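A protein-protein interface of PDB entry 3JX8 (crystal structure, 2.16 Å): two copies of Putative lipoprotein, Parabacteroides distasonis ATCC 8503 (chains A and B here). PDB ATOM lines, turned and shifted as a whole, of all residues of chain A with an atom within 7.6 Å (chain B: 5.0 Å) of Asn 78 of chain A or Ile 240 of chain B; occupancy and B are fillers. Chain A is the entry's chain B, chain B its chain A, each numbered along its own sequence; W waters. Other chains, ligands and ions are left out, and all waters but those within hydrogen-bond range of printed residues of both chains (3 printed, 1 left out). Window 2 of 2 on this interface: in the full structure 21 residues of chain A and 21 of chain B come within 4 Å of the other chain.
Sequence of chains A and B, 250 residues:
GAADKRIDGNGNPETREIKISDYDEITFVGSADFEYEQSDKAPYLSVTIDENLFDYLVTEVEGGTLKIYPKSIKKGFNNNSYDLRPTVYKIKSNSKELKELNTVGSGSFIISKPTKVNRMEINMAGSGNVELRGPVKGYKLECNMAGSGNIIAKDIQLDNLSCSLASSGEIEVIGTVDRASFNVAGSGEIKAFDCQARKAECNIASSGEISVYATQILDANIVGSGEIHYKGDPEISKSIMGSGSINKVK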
ATOM      1  N   THR A  27     -17.559 -30.538 -10.975  1.00  0.00           N
ATOM      2  CA  THR A  27     -17.075 -30.027 -12.238  1.00  0.00           C
ATOM      3  C   THR A  27     -17.467 -28.572 -12.309  1.00  0.00           C
ATOM      4  O   THR A  27     -18.642 -28.266 -12.401  1.00  0.00           O
ATOM      5  CB  THR A  27     -17.752 -30.743 -13.426  1.00  0.00           C
ATOM      6  OG1 THR A  27     -17.328 -32.103 -13.439  1.00  0.00           O
ATOM      7  CG2 THR A  27     -17.407 -30.081 -14.772  1.00  0.00           C
ATOM      8  N   VAL A  29     -16.716 -24.965 -14.329  1.00  0.00           N
ATOM      9  CA  VAL A  29     -16.065 -24.221 -15.407  1.00  0.00           C
ATOM     10  C   VAL A  29     -16.529 -22.787 -15.309  1.00  0.00           C
ATOM     11  O   VAL A  29     -17.733 -22.517 -15.274  1.00  0.00           O
ATOM     12  CB  VAL A  29     -16.464 -24.791 -16.781  1.00  0.00           C
ATOM     13  CG1 VAL A  29     -15.880 -23.951 -17.930  1.00  0.00           C
ATOM     14  CG2 VAL A  29     -16.117 -26.280 -16.874  1.00  0.00           C
ATOM     15  N   TYR A  69     -21.359 -25.022 -15.214  1.00  0.00           N
ATOM     16  CA  TYR A  69     -20.585 -24.617 -16.377  1.00  0.00           C
ATOM     17  C   TYR A  69     -21.472 -23.917 -17.395  1.00  0.00           C
ATOM     18  O   TYR A  69     -22.698 -24.130 -17.423  1.00  0.00           O
ATOM     19  CB  TYR A  69     -19.877 -25.838 -17.037  1.00  0.00           C
ATOM     20  CG  TYR A  69     -20.788 -26.983 -17.356  1.00  0.00           C
ATOM     21  CD1 TYR A  69     -21.543 -26.971 -18.508  1.00  0.00           C
ATOM     22  CD2 TYR A  69     -20.877 -28.097 -16.531  1.00  0.00           C
ATOM     23  CE1 TYR A  69     -22.377 -27.979 -18.820  1.00  0.00           C
ATOM     24  CE2 TYR A  69     -21.753 -29.152 -16.857  1.00  0.00           C
ATOM     25  CZ  TYR A  69     -22.504 -29.058 -17.982  1.00  0.00           C
ATOM     26  OH  TYR A  69     -23.401 -30.049 -18.349  1.00  0.00           O
ATOM     27  N   PRO A  70     -20.867 -23.084 -18.240  1.00  0.00           N
ATOM     28  CA  PRO A  70     -21.696 -22.501 -19.285  1.00  0.00           C
ATOM     29  C   PRO A  70     -22.171 -23.530 -20.288  1.00  0.00           C
ATOM     30  O   PRO A  70     -21.454 -24.494 -20.611  1.00  0.00           O
ATOM     31  CB  PRO A  70     -20.775 -21.498 -19.950  1.00  0.00           C
ATOM     32  CG  PRO A  70     -19.642 -21.307 -19.036  1.00  0.00           C
ATOM     33  CD  PRO A  70     -19.494 -22.558 -18.290  1.00  0.00           C
ATOM     34  N   LYS A  71     -23.398 -23.332 -20.757  1.00  0.00           N
ATOM     35  CA  LYS A  71     -23.985 -24.191 -21.768  1.00  0.00           C
ATOM     36  C   LYS A  71     -23.266 -24.176 -23.109  1.00  0.00           C
ATOM     37  O   LYS A  71     -22.619 -23.179 -23.508  1.00  0.00           O
ATOM     38  CB  LYS A  71     -25.454 -23.791 -22.034  1.00  0.00           C
ATOM     39  CG  LYS A  71     -26.398 -23.968 -20.855  1.00  0.00           C
ATOM     40  CD  LYS A  71     -27.836 -23.568 -21.263  1.00  0.00           C
ATOM     41  CE  LYS A  71     -28.797 -23.728 -20.141  1.00  0.00           C
ATOM     42  NZ  LYS A  71     -30.161 -23.184 -20.375  1.00  0.00           N
ATOM     43  N   SER A  72     -23.442 -25.276 -23.837  1.00  0.00           N
ATOM     44  CA  SER A  72     -23.046 -25.334 -25.236  1.00  0.00           C
ATOM     45  C   SER A  72     -23.861 -24.343 -26.028  1.00  0.00           C
ATOM     46  O   SER A  72     -25.039 -24.154 -25.755  1.00  0.00           O
ATOM     47  CB  SER A  72     -23.305 -26.716 -25.835  1.00  0.00           C
ATOM     48  OG  SER A  72     -22.493 -27.645 -25.203  1.00  0.00           O
ATOM     49  N   ILE A  73     -23.248 -23.753 -27.045  1.00  0.00           N
ATOM     50  CA  ILE A  73     -23.971 -22.793 -27.868  1.00  0.00           C
ATOM     51  C   ILE A  73     -25.110 -23.506 -28.561  1.00  0.00           C
ATOM     52  O   ILE A  73     -24.933 -24.565 -29.161  1.00  0.00           O
ATOM     53  CB  ILE A  73     -23.065 -22.082 -28.876  1.00  0.00           C
ATOM     54  CG1 ILE A  73     -21.961 -21.338 -28.108  1.00  0.00           C
ATOM     55  CG2 ILE A  73     -23.876 -21.094 -29.746  1.00  0.00           C
ATOM     56  CD1 ILE A  73     -21.049 -20.540 -28.985  1.00  0.00           C
ATOM     57  N   LYS A  74     -26.297 -22.923 -28.428  1.00  0.00           N
ATOM     58  CA  LYS A  74     -27.513 -23.427 -29.065  1.00  0.00           C
ATOM     59  C   LYS A  74     -27.274 -23.661 -30.558  1.00  0.00           C
ATOM     60  O   LYS A  74     -26.835 -22.777 -31.258  1.00  0.00           O
ATOM     61  CB  LYS A  74     -28.666 -22.440 -28.842  1.00  0.00           C
ATOM     62  CG  LYS A  74     -30.072 -22.961 -29.250  1.00  0.00           C
ATOM     63  CD  LYS A  74     -31.176 -22.342 -28.341  1.00  0.00           C
ATOM     64  N   LYS A  75     -27.485 -24.888 -31.000  1.00  0.00           N
ATOM     65  CA  LYS A  75     -27.297 -25.278 -32.374  1.00  0.00           C
ATOM     66  C   LYS A  75     -25.856 -25.182 -32.810  1.00  0.00           C
ATOM     67  O   LYS A  75     -25.591 -25.050 -33.992  1.00  0.00           O
ATOM     68  CB  LYS A  75     -28.177 -24.457 -33.328  1.00  0.00           C
ATOM     69  CG  LYS A  75     -29.676 -24.441 -32.995  1.00  0.00           C
ATOM     70  CD  LYS A  75     -30.330 -25.785 -33.273  1.00  0.00           C
ATOM     71  CE  LYS A  75     -31.875 -25.716 -33.165  1.00  0.00           C
ATOM     72  NZ  LYS A  75     -32.517 -24.884 -34.245  1.00  0.00           N
ATOM     73  N   GLY A  76     -24.913 -25.262 -31.881  1.00  0.00           N
ATOM     74  CA  GLY A  76     -23.521 -25.330 -32.252  1.00  0.00           C
ATOM     75  C   GLY A  76     -22.914 -26.710 -32.122  1.00  0.00           C
ATOM     76  O   GLY A  76     -21.694 -26.850 -32.205  1.00  0.00           O
ATOM     77  N   PHE A  77     -23.756 -27.712 -31.867  1.00  0.00           N
ATOM     78  CA  PHE A  77     -23.399 -29.127 -31.887  1.00  0.00           C
ATOM     79  C   PHE A  77     -22.409 -29.520 -30.810  1.00  0.00           C
ATOM     80  O   PHE A  77     -21.614 -30.421 -30.983  1.00  0.00           O
ATOM     81  CB  PHE A  77     -22.924 -29.528 -33.282  1.00  0.00           C
ATOM     82  CG  PHE A  77     -23.714 -28.876 -34.407  1.00  0.00           C
ATOM     83  CD1 PHE A  77     -25.080 -28.704 -34.320  1.00  0.00           C
ATOM     84  CD2 PHE A  77     -23.080 -28.422 -35.551  1.00  0.00           C
ATOM     85  CE1 PHE A  77     -25.800 -28.073 -35.344  1.00  0.00           C
ATOM     86  CE2 PHE A  77     -23.802 -27.828 -36.596  1.00  0.00           C
ATOM     87  CZ  PHE A  77     -25.151 -27.654 -36.479  1.00  0.00           C
ATOM     88  N   ASN A  78     -22.484 -28.840 -29.678  1.00  0.00           N
ATOM     89  CA  ASN A  78     -21.513 -28.969 -28.597  1.00  0.00           C
ATOM     90  C   ASN A  78     -20.054 -28.778 -29.041  1.00  0.00           C
ATOM     91  O   ASN A  78     -19.144 -29.288 -28.387  1.00  0.00           O
ATOM     92  CB  ASN A  78     -21.673 -30.320 -27.832  1.00  0.00           C
ATOM     93  CG  ASN A  78     -23.071 -30.518 -27.258  1.00  0.00           C
ATOM     94  OD1 ASN A  78     -23.688 -29.576 -26.772  1.00  0.00           O
ATOM     95  ND2 ASN A  78     -23.572 -31.745 -27.304  1.00  0.00           N
ATOM     96  N   ASN A  79     -19.816 -28.026 -30.107  1.00  0.00           N
ATOM     97  CA  ASN A  79     -18.442 -27.668 -30.487  1.00  0.00           C
ATOM     98  C   ASN A  79     -17.820 -26.515 -29.668  1.00  0.00           C
ATOM     99  O   ASN A  79     -16.611 -26.287 -29.731  1.00  0.00           O
ATOM    100  CB  ASN A  79     -18.405 -27.372 -31.982  1.00  0.00           C
ATOM    101  CG  ASN A  79     -18.627 -28.629 -32.811  1.00  0.00           C
ATOM    102  OD1 ASN A  79     -18.307 -29.731 -32.372  1.00  0.00           O
ATOM    103  ND2 ASN A  79     -19.187 -28.469 -33.995  1.00  0.00           N
ATOM    104  N   ASN A  80     -18.644 -25.820 -28.894  1.00  0.00           N
ATOM    105  CA  ASN A  80     -18.225 -24.700 -28.070  1.00  0.00           C
ATOM    106  C   ASN A  80     -19.337 -24.262 -27.157  1.00  0.00           C
ATOM    107  O   ASN A  80     -20.487 -24.641 -27.310  1.00  0.00           O
ATOM    108  CB  ASN A  80     -17.827 -23.509 -28.928  1.00  0.00           C
ATOM    109  CG  ASN A  80     -18.614 -23.450 -30.166  1.00  0.00           C
ATOM    110  OD1 ASN A  80     -19.868 -23.490 -30.123  1.00  0.00           O
ATOM    111  ND2 ASN A  80     -17.916 -23.484 -31.314  1.00  0.00           N
ATOM    112  N   SER A  81     -18.980 -23.432 -26.199  1.00  0.00           N
ATOM    113  CA  SER A  81     -19.923 -23.010 -25.190  1.00  0.00           C
ATOM    114  C   SER A  81     -19.935 -21.495 -25.129  1.00  0.00           C
ATOM    115  O   SER A  81     -19.082 -20.838 -25.710  1.00  0.00           O
ATOM    116  CB  SER A  81     -19.500 -23.625 -23.864  1.00  0.00           C
ATOM    117  OG  SER A  81     -18.177 -23.209 -23.613  1.00  0.00           O
ATOM    118  N   ILE B 222     -10.856 -32.085 -24.775  1.00  0.00           N
ATOM    119  CA  ILE B 222     -10.258 -30.836 -24.328  1.00  0.00           C
ATOM    120  C   ILE B 222     -10.708 -30.549 -22.907  1.00  0.00           C
ATOM    121  O   ILE B 222     -11.924 -30.594 -22.575  1.00  0.00           O
ATOM    122  CB  ILE B 222     -10.687 -29.630 -25.196  1.00  0.00           C
ATOM    123  CG1 ILE B 222     -10.419 -29.907 -26.686  1.00  0.00           C
ATOM    124  CG2 ILE B 222     -10.035 -28.329 -24.668  1.00  0.00           C
ATOM    125  CD1 ILE B 222     -10.991 -28.858 -27.657  1.00  0.00           C
ATOM    126  N   LYS B 238     -16.851 -36.226 -29.085  1.00  0.00           N
ATOM    127  CA  LYS B 238     -16.458 -34.889 -28.624  1.00  0.00           C
ATOM    128  C   LYS B 238     -16.509 -34.842 -27.110  1.00  0.00           C
ATOM    129  O   LYS B 238     -17.442 -35.364 -26.505  1.00  0.00           O
ATOM    130  CB  LYS B 238     -17.420 -33.853 -29.143  1.00  0.00           C
ATOM    131  CG  LYS B 238     -17.476 -33.743 -30.622  1.00  0.00           C
ATOM    132  CD  LYS B 238     -18.635 -32.835 -31.021  1.00  0.00           C
ATOM    133  CE  LYS B 238     -18.853 -32.768 -32.513  1.00  0.00           C
ATOM    134  NZ  LYS B 238     -20.063 -31.980 -32.808  1.00  0.00           N
ATOM    135  N   SER B 239     -15.523 -34.206 -26.490  1.00  0.00           N
ATOM    136  CA  SER B 239     -15.578 -33.964 -25.062  1.00  0.00           C
ATOM    137  C   SER B 239     -14.833 -32.687 -24.722  1.00  0.00           C
ATOM    138  O   SER B 239     -13.625 -32.600 -24.944  1.00  0.00           O
ATOM    139  CB  SER B 239     -14.970 -35.144 -24.363  1.00  0.00           C
ATOM    140  OG  SER B 239     -14.925 -34.863 -22.991  1.00  0.00           O
ATOM    141  N   ILE B 240     -15.552 -31.685 -24.233  1.00  0.00           N
ATOM    142  CA  ILE B 240     -14.966 -30.405 -23.869  1.00  0.00           C
ATOM    143  C   ILE B 240     -15.398 -29.971 -22.457  1.00  0.00           C
ATOM    144  O   ILE B 240     -16.582 -29.828 -22.178  1.00  0.00           O
ATOM    145  CB  ILE B 240     -15.379 -29.281 -24.822  1.00  0.00           C
ATOM    146  CG1 ILE B 240     -15.068 -29.635 -26.254  1.00  0.00           C
ATOM    147  CG2 ILE B 240     -14.694 -27.983 -24.415  1.00  0.00           C
ATOM    148  CD1 ILE B 240     -15.636 -28.636 -27.258  1.00  0.00           C
ATOM    149  N   MET B 241     -14.425 -29.757 -21.578  1.00  0.00           N
ATOM    150  CA  MET B 241     -14.657 -29.150 -20.272  1.00  0.00           C
ATOM    151  C   MET B 241     -13.854 -27.886 -20.269  1.00  0.00           C
ATOM    152  O   MET B 241     -12.610 -27.911 -20.188  1.00  0.00           O
ATOM    153  CB  MET B 241     -14.202 -30.079 -19.137  1.00  0.00           C
ATOM    154  CG  MET B 241     -14.690 -29.609 -17.807  1.00  0.00           C
ATOM    155  SD  MET B 241     -13.728 -30.519 -16.358  1.00  0.00           S
ATOM    156  CE  MET B 241     -14.651 -32.264 -16.566  1.00  0.00           C
ATOM    157  N   GLY B 242     -14.530 -26.773 -20.413  1.00  0.00           N
ATOM    158  CA  GLY B 242     -13.854 -25.477 -20.486  1.00  0.00           C
ATOM    159  C   GLY B 242     -14.360 -24.649 -21.645  1.00  0.00           C
ATOM    160  O   GLY B 242     -15.356 -24.982 -22.250  1.00  0.00           O
ATOM    161  N   GLY B 244     -12.754 -24.158 -24.483  1.00  0.00           N
ATOM    162  CA  GLY B 244     -12.176 -24.612 -25.737  1.00  0.00           C
ATOM    163  C   GLY B 244     -13.196 -24.981 -26.794  1.00  0.00           C
ATOM    164  O   GLY B 244     -14.416 -24.868 -26.590  1.00  0.00           O
ATOM    165  N   SER B 245     -12.703 -25.421 -27.945  1.00  0.00           N
ATOM    166  CA  SER B 245     -13.581 -25.703 -29.054  1.00  0.00           C
ATOM    167  C   SER B 245     -13.003 -26.655 -30.072  1.00  0.00           C
ATOM    168  O   SER B 245     -11.795 -26.825 -30.177  1.00  0.00           O
ATOM    169  CB  SER B 245     -13.994 -24.394 -29.739  1.00  0.00           C
ATOM    170  OG  SER B 245     -12.896 -23.866 -30.409  1.00  0.00           O
ATOM    171  N   ILE B 246     -13.909 -27.289 -30.784  1.00  0.00           N
ATOM    172  CA  ILE B 246     -13.627 -28.242 -31.837  1.00  0.00           C
ATOM    173  C   ILE B 246     -14.200 -27.664 -33.105  1.00  0.00           C
ATOM    174  O   ILE B 246     -15.337 -27.192 -33.083  1.00  0.00           O
ATOM    175  CB  ILE B 246     -14.328 -29.596 -31.559  1.00  0.00           C
ATOM    176  CG1 ILE B 246     -13.683 -30.280 -30.353  1.00  0.00           C
ATOM    177  CG2 ILE B 246     -14.251 -30.540 -32.772  1.00  0.00           C
ATOM    178  CD1 ILE B 246     -14.468 -31.456 -29.820  1.00  0.00           C
HETATM  179  O   HOH W   1     -16.458 -24.799 -24.708  1.00  0.00           O
HETATM  180  O   HOH W   2     -16.252 -24.529 -33.427  1.00  0.00           O
HETATM  181  O   HOH W   3     -16.194 -22.178 -26.828  1.00  0.00           O
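Printed residues of chain B within 4 Å of Thr 27 of chain A: Met 241 (3.9 Å).
Asn 78 of chain A touches just one residue of chain B: Ile 240 (3.7 Å).
Of the printed residues of chain B, Ser 81 of chain A touches Gly 242.
Printed residues of chain A within 4 Å of Lys 238 of chain B: Phe 77 (2.9 Å) and Asn 79 (2.9 Å).
Ser 239 of chain B touches none of the printed residues of chain A.
Ile 240 of chain B touches two residues of chain A.
Printed residues of chain A within 4 Å of Met 241 of chain B: Thr 27 (3.9 Å) and Val 29 (3.7 Å).
Printed residues of chain A within 4 Å of Ser 245 of chain B: Asn 79 (3.2 Å).
The nearest printed residue of chain A that does not touch Ile 246 of chain B is Asn 80 of chain A (4.9 Å).
The side-chain amino group of Lys 238 of chain B lies within hydrogen-bond range of the side-chain amide oxygen of Asn 79 of chain A, 2.9 Å away.
The side-chain amino group of Lys 238 of chain B sits at hydrogen-bond distance from the backbone carbonyl oxygen of Phe 77 of chain A, 2.9 Å away.
O of Asn 79 of chain A lies within hydrogen-bond range of N of Ile 246 of chain B, 3.1 Å away.
The side-chain hydroxyl (OG) of Ser 72 of chain A sits at hydrogen-bond distance from the side-chain amide oxygen (OD1) of Asn 78 of chain A (2.8 Å).
N of Met 241 of chain B lies within hydrogen-bond range of O of Ile 222 of chain B (2.8 Å).
The backbone carbonyl oxygen of Gly 76 of chain A lies close to the side-chain amide nitrogen of Asn 79 of chain A, at 3.5 Å.
Printed residues of chain A that touch a printed residue of chain B: Thr 27, Val 29, Phe 77, Asn 78, Asn 79 and Ser 81.
Hydrophobic or aromatic side chains of chain A that line the printed part of chain B: Val 29 and Phe 77.
Of the 9 printed residues of chain B, 6 touch a printed residue of chain A.
Printed residues of chain B that touch a printed residue of chain A: Lys 238, Ile 240, Met 241, Gly 242, Ser 245 and Ile 246.
Thr 27 of chain A touches Met 241 of chain B (CG2 to CE, 3.9 Å).
Val 29 of chain A touches Met 241 of chain B.
Val 29 of chain A touches Gly 242 of chain B (CG1 to CA, 3.6 Å).
Ile 240 of chain B touches Asn 78 of chain A (CD1 to O, 3.7 Å).
O of Asn 79 of chain A touches CD1 of Ile 240 of chain B (3.5 Å).
CA of Ser 245 of chain B touches O of Asn 79 of chain A, 3.2 Å away.
Ser 81 of chain A touches Gly 242 of chain B.
Water W1 lies within hydrogen-bond range of the side-chain hydroxyl (OG) of Ser 81 of chain A (2.6 Å), the backbone carbonyl oxygen (O) of Gly 242 of chain B (2.7 Å) and the backbone carbonyl oxygen (O) of Gly 244 of chain B (2.8 Å).
Water W2 lies within hydrogen-bond range of the backbone carbonyl oxygen (O) of Ile 246 of chain B (2.8 Å) and the side-chain amide nitrogen (ND2) of Asn 80 of chain A (2.9 Å).
Water W3 bridges N of Ser 81 of chain A (3.1 Å) and O of Gly 244 of chain B (3.2 Å).
No position is printed for both chains.
Of the 10 pairs that touch across the chains among the printed residues, none has its exchanged pair printed and touching as well.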
